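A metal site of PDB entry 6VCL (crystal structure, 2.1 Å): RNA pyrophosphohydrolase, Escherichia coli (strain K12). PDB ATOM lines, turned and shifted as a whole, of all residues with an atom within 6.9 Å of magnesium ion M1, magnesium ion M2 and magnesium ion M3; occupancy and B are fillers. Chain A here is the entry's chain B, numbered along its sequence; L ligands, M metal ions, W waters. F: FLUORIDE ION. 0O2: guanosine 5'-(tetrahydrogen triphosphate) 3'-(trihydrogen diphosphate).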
ATOM      1  N   ARG A   9      29.826   3.230 -20.261  1.00  0.00           N
ATOM      2  CA  ARG A   9      28.793   2.204 -20.398  1.00  0.00           C
ATOM      3  C   ARG A   9      27.919   2.166 -19.140  1.00  0.00           C
ATOM      4  O   ARG A   9      28.450   1.964 -18.044  1.00  0.00           O
ATOM      5  CB  ARG A   9      29.427   0.836 -20.641  1.00  0.00           C
ATOM      6  CG  ARG A   9      28.383  -0.264 -20.923  1.00  0.00           C
ATOM      7  CD  ARG A   9      28.996  -1.530 -21.503  1.00  0.00           C
ATOM      8  NE  ARG A   9      29.424  -2.396 -20.421  1.00  0.00           N
ATOM      9  CZ  ARG A   9      28.937  -3.598 -20.153  1.00  0.00           C
ATOM     10  NH1 ARG A   9      28.004  -4.170 -20.922  1.00  0.00           N
ATOM     11  NH2 ARG A   9      29.413  -4.255 -19.112  1.00  0.00           N
ATOM     12  N   ASN A  11      25.897   0.660 -16.173  1.00  0.00           N
ATOM     13  CA  ASN A  11      26.302  -0.585 -15.526  1.00  0.00           C
ATOM     14  C   ASN A  11      25.659  -0.650 -14.149  1.00  0.00           C
ATOM     15  O   ASN A  11      25.361   0.375 -13.547  1.00  0.00           O
ATOM     16  CB  ASN A  11      27.839  -0.648 -15.444  1.00  0.00           C
ATOM     17  CG  ASN A  11      28.353  -1.970 -14.918  1.00  0.00           C
ATOM     18  OD1 ASN A  11      28.252  -2.246 -13.724  1.00  0.00           O
ATOM     19  ND2 ASN A  11      28.908  -2.803 -15.806  1.00  0.00           N
ATOM     20  N   VAL A  12      25.415  -1.877 -13.668  1.00  0.00           N
ATOM     21  CA  VAL A  12      24.882  -2.074 -12.314  1.00  0.00           C
ATOM     22  C   VAL A  12      25.806  -3.020 -11.557  1.00  0.00           C
ATOM     23  O   VAL A  12      26.270  -4.030 -12.091  1.00  0.00           O
ATOM     24  CB  VAL A  12      23.428  -2.597 -12.323  1.00  0.00           C
ATOM     25  CG1 VAL A  12      22.469  -1.542 -12.871  1.00  0.00           C
ATOM     26  CG2 VAL A  12      23.302  -3.921 -13.092  1.00  0.00           C
ATOM     27  N   ARG A  28      36.713 -13.964 -11.058  1.00  0.00           N
ATOM     28  CA  ARG A  28      36.560 -13.842 -12.502  1.00  0.00           C
ATOM     29  C   ARG A  28      36.982 -15.119 -13.217  1.00  0.00           C
ATOM     30  O   ARG A  28      38.089 -15.637 -13.012  1.00  0.00           O
ATOM     31  CB  ARG A  28      37.418 -12.691 -13.029  1.00  0.00           C
ATOM     32  CG  ARG A  28      36.752 -11.371 -13.161  1.00  0.00           C
ATOM     33  CD  ARG A  28      37.742 -10.384 -13.750  1.00  0.00           C
ATOM     34  NE  ARG A  28      37.509 -10.173 -15.179  1.00  0.00           N
ATOM     35  CZ  ARG A  28      36.539  -9.403 -15.655  1.00  0.00           C
ATOM     36  NH1 ARG A  28      35.703  -8.787 -14.822  1.00  0.00           N
ATOM     37  NH2 ARG A  28      36.386  -9.257 -16.973  1.00  0.00           N
ATOM     38  N   GLN A  35      36.029  -9.881  -7.357  1.00  0.00           N
ATOM     39  CA  GLN A  35      35.242  -8.665  -7.498  1.00  0.00           C
ATOM     40  C   GLN A  35      33.799  -8.930  -7.085  1.00  0.00           C
ATOM     41  O   GLN A  35      33.394 -10.070  -6.822  1.00  0.00           O
ATOM     42  CB  GLN A  35      35.288  -8.136  -8.943  1.00  0.00           C
ATOM     43  CG  GLN A  35      34.604  -9.093  -9.926  1.00  0.00           C
ATOM     44  CD  GLN A  35      34.557  -8.545 -11.338  1.00  0.00           C
ATOM     45  OE1 GLN A  35      35.497  -8.719 -12.097  1.00  0.00           O
ATOM     46  NE2 GLN A  35      33.465  -7.862 -11.689  1.00  0.00           N
ATOM     47  N   PHE A  36      33.025  -7.849  -7.036  1.00  0.00           N
ATOM     48  CA  PHE A  36      31.580  -8.004  -6.952  1.00  0.00           C
ATOM     49  C   PHE A  36      31.004  -8.243  -8.352  1.00  0.00           C
ATOM     50  O   PHE A  36      31.525  -7.720  -9.333  1.00  0.00           O
ATOM     51  CB  PHE A  36      30.916  -6.764  -6.360  1.00  0.00           C
ATOM     52  CG  PHE A  36      31.258  -6.473  -4.912  1.00  0.00           C
ATOM     53  CD1 PHE A  36      31.191  -7.463  -3.944  1.00  0.00           C
ATOM     54  CD2 PHE A  36      31.616  -5.178  -4.542  1.00  0.00           C
ATOM     55  CE1 PHE A  36      31.470  -7.163  -2.587  1.00  0.00           C
ATOM     56  CE2 PHE A  36      31.886  -4.857  -3.194  1.00  0.00           C
ATOM     57  CZ  PHE A  36      31.828  -5.860  -2.211  1.00  0.00           C
ATOM     58  N   PRO A  37      29.865  -8.937  -8.451  1.00  0.00           N
ATOM     59  CA  PRO A  37      29.173  -9.015  -9.737  1.00  0.00           C
ATOM     60  C   PRO A  37      28.766  -7.621 -10.203  1.00  0.00           C
ATOM     61  O   PRO A  37      28.398  -6.763  -9.395  1.00  0.00           O
ATOM     62  CB  PRO A  37      27.937  -9.867  -9.426  1.00  0.00           C
ATOM     63  CG  PRO A  37      28.221 -10.529  -8.130  1.00  0.00           C
ATOM     64  CD  PRO A  37      29.084  -9.545  -7.370  1.00  0.00           C
ATOM     65  N   GLN A  38      28.815  -7.415 -11.517  1.00  0.00           N
ATOM     66  CA  GLN A  38      28.348  -6.180 -12.140  1.00  0.00           C
ATOM     67  C   GLN A  38      28.077  -6.475 -13.611  1.00  0.00           C
ATOM     68  O   GLN A  38      28.593  -7.445 -14.157  1.00  0.00           O
ATOM     69  CB  GLN A  38      29.392  -5.069 -11.994  1.00  0.00           C
ATOM     70  CG  GLN A  38      30.643  -5.395 -12.789  1.00  0.00           C
ATOM     71  CD  GLN A  38      31.623  -4.240 -12.837  1.00  0.00           C
ATOM     72  OE1 GLN A  38      32.052  -3.734 -11.804  1.00  0.00           O
ATOM     73  NE2 GLN A  38      31.969  -3.815 -14.052  1.00  0.00           N
ATOM     74  N   GLY A  39      27.282  -5.615 -14.244  1.00  0.00           N
ATOM     75  CA  GLY A  39      27.040  -5.857 -15.667  1.00  0.00           C
ATOM     76  C   GLY A  39      26.282  -4.738 -16.325  1.00  0.00           C
ATOM     77  O   GLY A  39      25.737  -3.831 -15.676  1.00  0.00           O
ATOM     78  N   GLY A  40      26.246  -4.808 -17.659  1.00  0.00           N
ATOM     79  CA  GLY A  40      25.709  -3.711 -18.447  1.00  0.00           C
ATOM     80  C   GLY A  40      24.184  -3.722 -18.459  1.00  0.00           C
ATOM     81  O   GLY A  40      23.538  -4.769 -18.549  1.00  0.00           O
ATOM     82  N   ILE A  41      23.616  -2.534 -18.324  1.00  0.00           N
ATOM     83  CA  ILE A  41      22.196  -2.311 -18.587  1.00  0.00           C
ATOM     84  C   ILE A  41      21.942  -2.438 -20.084  1.00  0.00           C
ATOM     85  O   ILE A  41      22.621  -1.778 -20.893  1.00  0.00           O
ATOM     86  CB  ILE A  41      21.762  -0.935 -18.080  1.00  0.00           C
ATOM     87  CG1 ILE A  41      22.162  -0.759 -16.633  1.00  0.00           C
ATOM     88  CG2 ILE A  41      20.240  -0.714 -18.315  1.00  0.00           C
ATOM     89  CD1 ILE A  41      21.948   0.641 -16.110  1.00  0.00           C
ATOM     90  N   ASN A  42      20.962  -3.256 -20.461  1.00  0.00           N
ATOM     91  CA  ASN A  42      20.658  -3.488 -21.868  1.00  0.00           C
ATOM     92  C   ASN A  42      19.581  -2.531 -22.339  1.00  0.00           C
ATOM     93  O   ASN A  42      18.888  -1.892 -21.538  1.00  0.00           O
ATOM     94  CB  ASN A  42      20.255  -4.941 -22.086  1.00  0.00           C
ATOM     95  CG  ASN A  42      21.418  -5.898 -21.950  1.00  0.00           C
ATOM     96  OD1 ASN A  42      22.574  -5.477 -21.992  1.00  0.00           O
ATOM     97  ND2 ASN A  42      21.129  -7.183 -21.788  1.00  0.00           N
ATOM     98  N   ARG A  53      18.566  -9.286 -13.831  1.00  0.00           N
ATOM     99  CA  ARG A  53      19.007 -10.152 -14.918  1.00  0.00           C
ATOM    100  C   ARG A  53      20.470 -10.560 -14.743  1.00  0.00           C
ATOM    101  O   ARG A  53      20.802 -11.752 -14.811  1.00  0.00           O
ATOM    102  CB  ARG A  53      18.818  -9.461 -16.273  1.00  0.00           C
ATOM    103  CG  ARG A  53      19.316 -10.308 -17.456  1.00  0.00           C
ATOM    104  CD  ARG A  53      19.156  -9.574 -18.785  1.00  0.00           C
ATOM    105  NE  ARG A  53      19.667  -8.211 -18.686  1.00  0.00           N
ATOM    106  CZ  ARG A  53      20.950  -7.889 -18.589  1.00  0.00           C
ATOM    107  NH1 ARG A  53      21.289  -6.614 -18.490  1.00  0.00           N
ATOM    108  NH2 ARG A  53      21.895  -8.829 -18.593  1.00  0.00           N
ATOM    109  N   GLU A  54      21.355  -9.588 -14.522  1.00  0.00           N
ATOM    110  CA  GLU A  54      22.758  -9.938 -14.342  1.00  0.00           C
ATOM    111  C   GLU A  54      22.934 -10.829 -13.122  1.00  0.00           C
ATOM    112  O   GLU A  54      23.710 -11.789 -13.158  1.00  0.00           O
ATOM    113  CB  GLU A  54      23.616  -8.680 -14.209  1.00  0.00           C
ATOM    114  CG  GLU A  54      23.713  -7.885 -15.486  1.00  0.00           C
ATOM    115  CD  GLU A  54      24.694  -8.482 -16.487  1.00  0.00           C
ATOM    116  OE1 GLU A  54      25.558  -9.296 -16.073  1.00  0.00           O
ATOM    117  OE2 GLU A  54      24.606  -8.101 -17.676  1.00  0.00           O
ATOM    118  N   GLU A  57      22.107 -14.264 -14.188  1.00  0.00           N
ATOM    119  CA  GLU A  57      23.109 -14.719 -15.170  1.00  0.00           C
ATOM    120  C   GLU A  57      24.455 -15.039 -14.521  1.00  0.00           C
ATOM    121  O   GLU A  57      25.154 -15.962 -14.958  1.00  0.00           O
ATOM    122  CB  GLU A  57      23.327 -13.642 -16.246  1.00  0.00           C
ATOM    123  CG  GLU A  57      22.108 -13.248 -17.097  1.00  0.00           C
ATOM    124  CD  GLU A  57      22.461 -12.126 -18.095  1.00  0.00           C
ATOM    125  OE1 GLU A  57      23.540 -11.481 -18.004  1.00  0.00           O
ATOM    126  OE2 GLU A  57      21.643 -11.881 -18.982  1.00  0.00           O
ATOM    127  N   GLU A  58      24.864 -14.245 -13.533  1.00  0.00           N
ATOM    128  CA  GLU A  58      26.224 -14.347 -12.999  1.00  0.00           C
ATOM    129  C   GLU A  58      26.298 -15.205 -11.747  1.00  0.00           C
ATOM    130  O   GLU A  58      27.253 -15.970 -11.585  1.00  0.00           O
ATOM    131  CB  GLU A  58      26.772 -12.942 -12.716  1.00  0.00           C
ATOM    132  CG  GLU A  58      26.942 -12.093 -14.006  1.00  0.00           C
ATOM    133  CD  GLU A  58      27.827 -10.848 -13.841  1.00  0.00           C
ATOM    134  OE1 GLU A  58      28.314 -10.592 -12.713  1.00  0.00           O
ATOM    135  OE2 GLU A  58      28.071 -10.149 -14.843  1.00  0.00           O
ATOM    136  N   THR A 119      28.108 -18.373 -20.915  1.00  0.00           N
ATOM    137  CA  THR A 119      29.386 -17.673 -20.784  1.00  0.00           C
ATOM    138  C   THR A 119      29.492 -17.163 -19.342  1.00  0.00           C
ATOM    139  O   THR A 119      29.193 -15.993 -19.064  1.00  0.00           O
ATOM    140  CB  THR A 119      29.438 -16.515 -21.779  1.00  0.00           C
ATOM    141  OG1 THR A 119      28.227 -15.769 -21.625  1.00  0.00           O
ATOM    142  CG2 THR A 119      29.491 -17.048 -23.199  1.00  0.00           C
ATOM    143  N   GLU A 121      30.693 -15.554 -16.001  1.00  0.00           N
ATOM    144  CA  GLU A 121      31.722 -14.571 -15.690  1.00  0.00           C
ATOM    145  C   GLU A 121      32.540 -14.926 -14.461  1.00  0.00           C
ATOM    146  O   GLU A 121      33.642 -14.382 -14.296  1.00  0.00           O
ATOM    147  CB  GLU A 121      31.103 -13.193 -15.503  1.00  0.00           C
ATOM    148  CG  GLU A 121      30.770 -12.619 -16.854  1.00  0.00           C
ATOM    149  CD  GLU A 121      29.977 -11.352 -16.779  1.00  0.00           C
ATOM    150  OE1 GLU A 121      30.508 -10.318 -16.248  1.00  0.00           O
ATOM    151  OE2 GLU A 121      28.833 -11.395 -17.284  1.00  0.00           O
ATOM    152  N   PHE A 122      32.064 -15.845 -13.630  1.00  0.00           N
ATOM    153  CA  PHE A 122      32.752 -16.247 -12.415  1.00  0.00           C
ATOM    154  C   PHE A 122      32.887 -17.764 -12.358  1.00  0.00           C
ATOM    155  O   PHE A 122      32.052 -18.498 -12.886  1.00  0.00           O
ATOM    156  CB  PHE A 122      32.010 -15.744 -11.167  1.00  0.00           C
ATOM    157  CG  PHE A 122      31.827 -14.240 -11.133  1.00  0.00           C
ATOM    158  CD1 PHE A 122      32.923 -13.390 -11.064  1.00  0.00           C
ATOM    159  CD2 PHE A 122      30.552 -13.687 -11.112  1.00  0.00           C
ATOM    160  CE1 PHE A 122      32.766 -12.006 -11.012  1.00  0.00           C
ATOM    161  CE2 PHE A 122      30.386 -12.303 -11.061  1.00  0.00           C
ATOM    162  CZ  PHE A 122      31.512 -11.455 -11.003  1.00  0.00           C
HETATM  163  F     F L   1      28.403  -8.573 -16.973  1.00  0.00           F
HETATM  164  PD  0O2 L   2      38.892  -9.395 -20.501  1.00  0.00           P
HETATM  165  O1D 0O2 L   2      39.281 -10.226 -21.695  1.00  0.00           O
HETATM  166  O2D 0O2 L   2      40.096  -9.281 -19.598  1.00  0.00           O
HETATM  167  O3D 0O2 L   2      37.715 -10.024 -19.741  1.00  0.00           O
HETATM  168  PG  0O2 L   2      30.849  -6.243 -17.111  1.00  0.00           P
HETATM  169  O1G 0O2 L   2      30.906  -7.360 -16.096  1.00  0.00           O
HETATM  170  O2G 0O2 L   2      29.592  -6.375 -17.996  1.00  0.00           O
HETATM  171  O3G 0O2 L   2      30.799  -4.904 -16.400  1.00  0.00           O
HETATM  172  PB  0O2 L   2      33.637  -6.383 -18.007  1.00  0.00           P
HETATM  173  O1B 0O2 L   2      34.337  -6.260 -19.341  1.00  0.00           O
HETATM  174  O2B 0O2 L   2      34.092  -7.663 -17.239  1.00  0.00           O
HETATM  175  O3B 0O2 L   2      32.062  -6.416 -18.148  1.00  0.00           O
HETATM  176  O3A 0O2 L   2      33.882  -5.008 -17.090  1.00  0.00           O
HETATM  177  PA  0O2 L   2      35.179  -4.543 -16.114  1.00  0.00           P
HETATM  178  O1A 0O2 L   2      35.125  -3.034 -16.064  1.00  0.00           O
HETATM  179  O2A 0O2 L   2      35.034  -5.215 -14.722  1.00  0.00           O
HETATM  180  O5' 0O2 L   2      36.468  -5.126 -16.822  1.00  0.00           O
HETATM  181  C5' 0O2 L   2      36.975  -4.468 -17.993  1.00  0.00           C
HETATM  182  C4' 0O2 L   2      38.440  -4.799 -18.202  1.00  0.00           C
HETATM  183  O4' 0O2 L   2      39.133  -4.722 -16.930  1.00  0.00           O
HETATM  184  C3' 0O2 L   2      38.634  -6.212 -18.725  1.00  0.00           C
HETATM  185  O3' 0O2 L   2      39.767  -6.273 -19.607  1.00  0.00           O
HETATM  186  C2' 0O2 L   2      38.917  -6.996 -17.440  1.00  0.00           C
HETATM  187  O2' 0O2 L   2      39.710  -8.153 -17.738  1.00  0.00           O
HETATM  188  C1' 0O2 L   2      39.746  -5.956 -16.624  1.00  0.00           C
HETATM  189  N9  0O2 L   2      39.528  -6.257 -15.223  1.00  0.00           N
HETATM  190  C8  0O2 L   2      38.396  -6.308 -14.504  1.00  0.00           C
HETATM  191  N7  0O2 L   2      38.547  -6.633 -13.208  1.00  0.00           N
HETATM  192  C5  0O2 L   2      39.880  -6.795 -13.098  1.00  0.00           C
HETATM  193  C6  0O2 L   2      40.699  -7.146 -12.012  1.00  0.00           C
HETATM  194  O6  0O2 L   2      40.166  -7.362 -10.913  1.00  0.00           O
HETATM  195  N1  0O2 L   2      42.031  -7.260 -12.126  1.00  0.00           N
HETATM  196  C2  0O2 L   2      42.514  -7.017 -13.352  1.00  0.00           C
HETATM  197  N2  0O2 L   2      43.849  -7.113 -13.504  1.00  0.00           N
HETATM  198  N3  0O2 L   2      41.836  -6.685 -14.455  1.00  0.00           N
HETATM  199  C4  0O2 L   2      40.484  -6.569 -14.328  1.00  0.00           C
HETATM  200  PC  0O2 L   2      39.392  -6.534 -21.138  1.00  0.00           P
HETATM  201  O1C 0O2 L   2      38.537  -5.412 -21.711  1.00  0.00           O
HETATM  202  O2C 0O2 L   2      40.656  -6.727 -21.949  1.00  0.00           O
HETATM  203  O3C 0O2 L   2      38.513  -7.936 -21.042  1.00  0.00           O
HETATM  204 MG    MG M   1      27.163 -10.120 -17.036  1.00  0.00          MG
HETATM  205 MG    MG M   2      25.710  -8.212 -19.345  1.00  0.00          MG
HETATM  206 MG    MG M   3      29.533  -8.684 -15.319  1.00  0.00          MG
HETATM  207 MG    MG M   4      28.647  -7.902 -18.727  1.00  0.00          MG
HETATM  208  O   HOH W   1      27.051  -6.855 -18.840  1.00  0.00           O
HETATM  209  O   HOH W   2      25.962 -11.860 -17.010  1.00  0.00           O
HETATM  210  O   HOH W   3      26.362  -8.162 -21.475  1.00  0.00           O
HETATM  211  O   HOH W   4      30.732  -9.376 -13.536  1.00  0.00           O
HETATM  212  O   HOH W   5      27.000  -9.583 -19.011  1.00  0.00           O
HETATM  213  O   HOH W   6      24.434  -6.642 -19.943  1.00  0.00           O
HETATM  214  O   HOH W   7      24.536 -10.003 -20.181  1.00  0.00           O
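Magnesium ion M1 is bound by a fluorine (F) of F L1, the side-chain carboxylate of Glu 54, water W5, water W2, the side-chain carboxylate of Glu 121 and the side-chain carboxylate of Glu 58.
The side-chain carboxylate (OE2) of Glu 54 sits close to the guanidinium group (NH2) of Arg 53, 3.0 Å away.
The backbone carbonyl oxygen (O) of Gly 40 sits at hydrogen-bond distance from the guanidinium group (NH1) of Arg 53 (2.9 Å).
The guanidinium group (NH1) of Arg 53 sits close to the side-chain amide nitrogen (ND2) of Asn 42, at 3.4 Å.
The guanidinium group of Arg 53 lies within salt-bridge range of the side-chain carboxylate of Glu 57, 3.1 Å away.
The backbone NH of Val 12 lies within hydrogen-bond range of the backbone carbonyl oxygen of Gly 39, 2.8 Å away.
The backbone carbonyl oxygen (O) of Gly 39 sits close to the side-chain amide nitrogen (ND2) of Asn 11.
Water W6 lies within hydrogen-bond range of the backbone carbonyl oxygen of Gly 40 (2.5 Å), the side-chain amide oxygen of Asn 42 (3.0 Å) and the guanidinium group of Arg 53 (3.5 Å).
Water W7 lies within hydrogen-bond range of the side-chain carboxylate (OE1) of Glu 57 (2.8 Å) and the guanidinium group (NH2) of Arg 53 (3.3 Å).
Water W4 bridges the side-chain carboxylate (OE1) of Glu 58 (2.8 Å) and the backbone NH (N) of Gln 38 (3.4 Å).
NE2 of Gln 38 sits at hydrogen-bond distance from O3G of 0O2 L2, 2.8 Å away.
NH2 of Arg 28 lies within salt-bridge range of O2B of 0O2 L2.
An oxygen (O3G) of 0O2 L2 is in salt-bridge range of the guanidinium group (NH2) of Arg 9 (3.1 Å).
An oxygen (O3G) of 0O2 L2 lies within hydrogen-bond range of the side-chain amide nitrogen (ND2) of Asn 11.
Merely in contact with magnesium ion M3: Gly 39 (3.8 Å).
Of the 19 residues printed, 4 come within 4 Å of magnesium ion M3.
Along chain A the residues within 4 Å of magnesium ion M3 span positions 38 to 121.
Magnesium ion M3 is bound by O of Gln 38 (1.9 Å), F of F L1 (2.0 Å), O1G of 0O2 L2 (2.1 Å), OE1 of Glu 121 (2.1 Å), OE2 of Glu 58 (2.1 Å) and water W4 (2.3 Å).
Residues that only touch magnesium ion M2: Gly 40 (3.8 Å) and Arg 53 (3.9 Å).
Within 4 Å of magnesium ion M2: Gly 40, Arg 53 and Glu 54.
Magnesium ion M2 is bound by water W5 (1.9 Å), water W1 (2.0 Å), OE2 of Glu 54 (2.0 Å), water W6 (2.1 Å), water W3 (2.2 Å) and water W7 (2.3 Å).
Residues that only touch magnesium ion M1: Glu 57 (3.99 Å).
Four residues have an atom within 4 Å of magnesium ion M1: Glu 54, Glu 57, Glu 58 and Glu 121.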
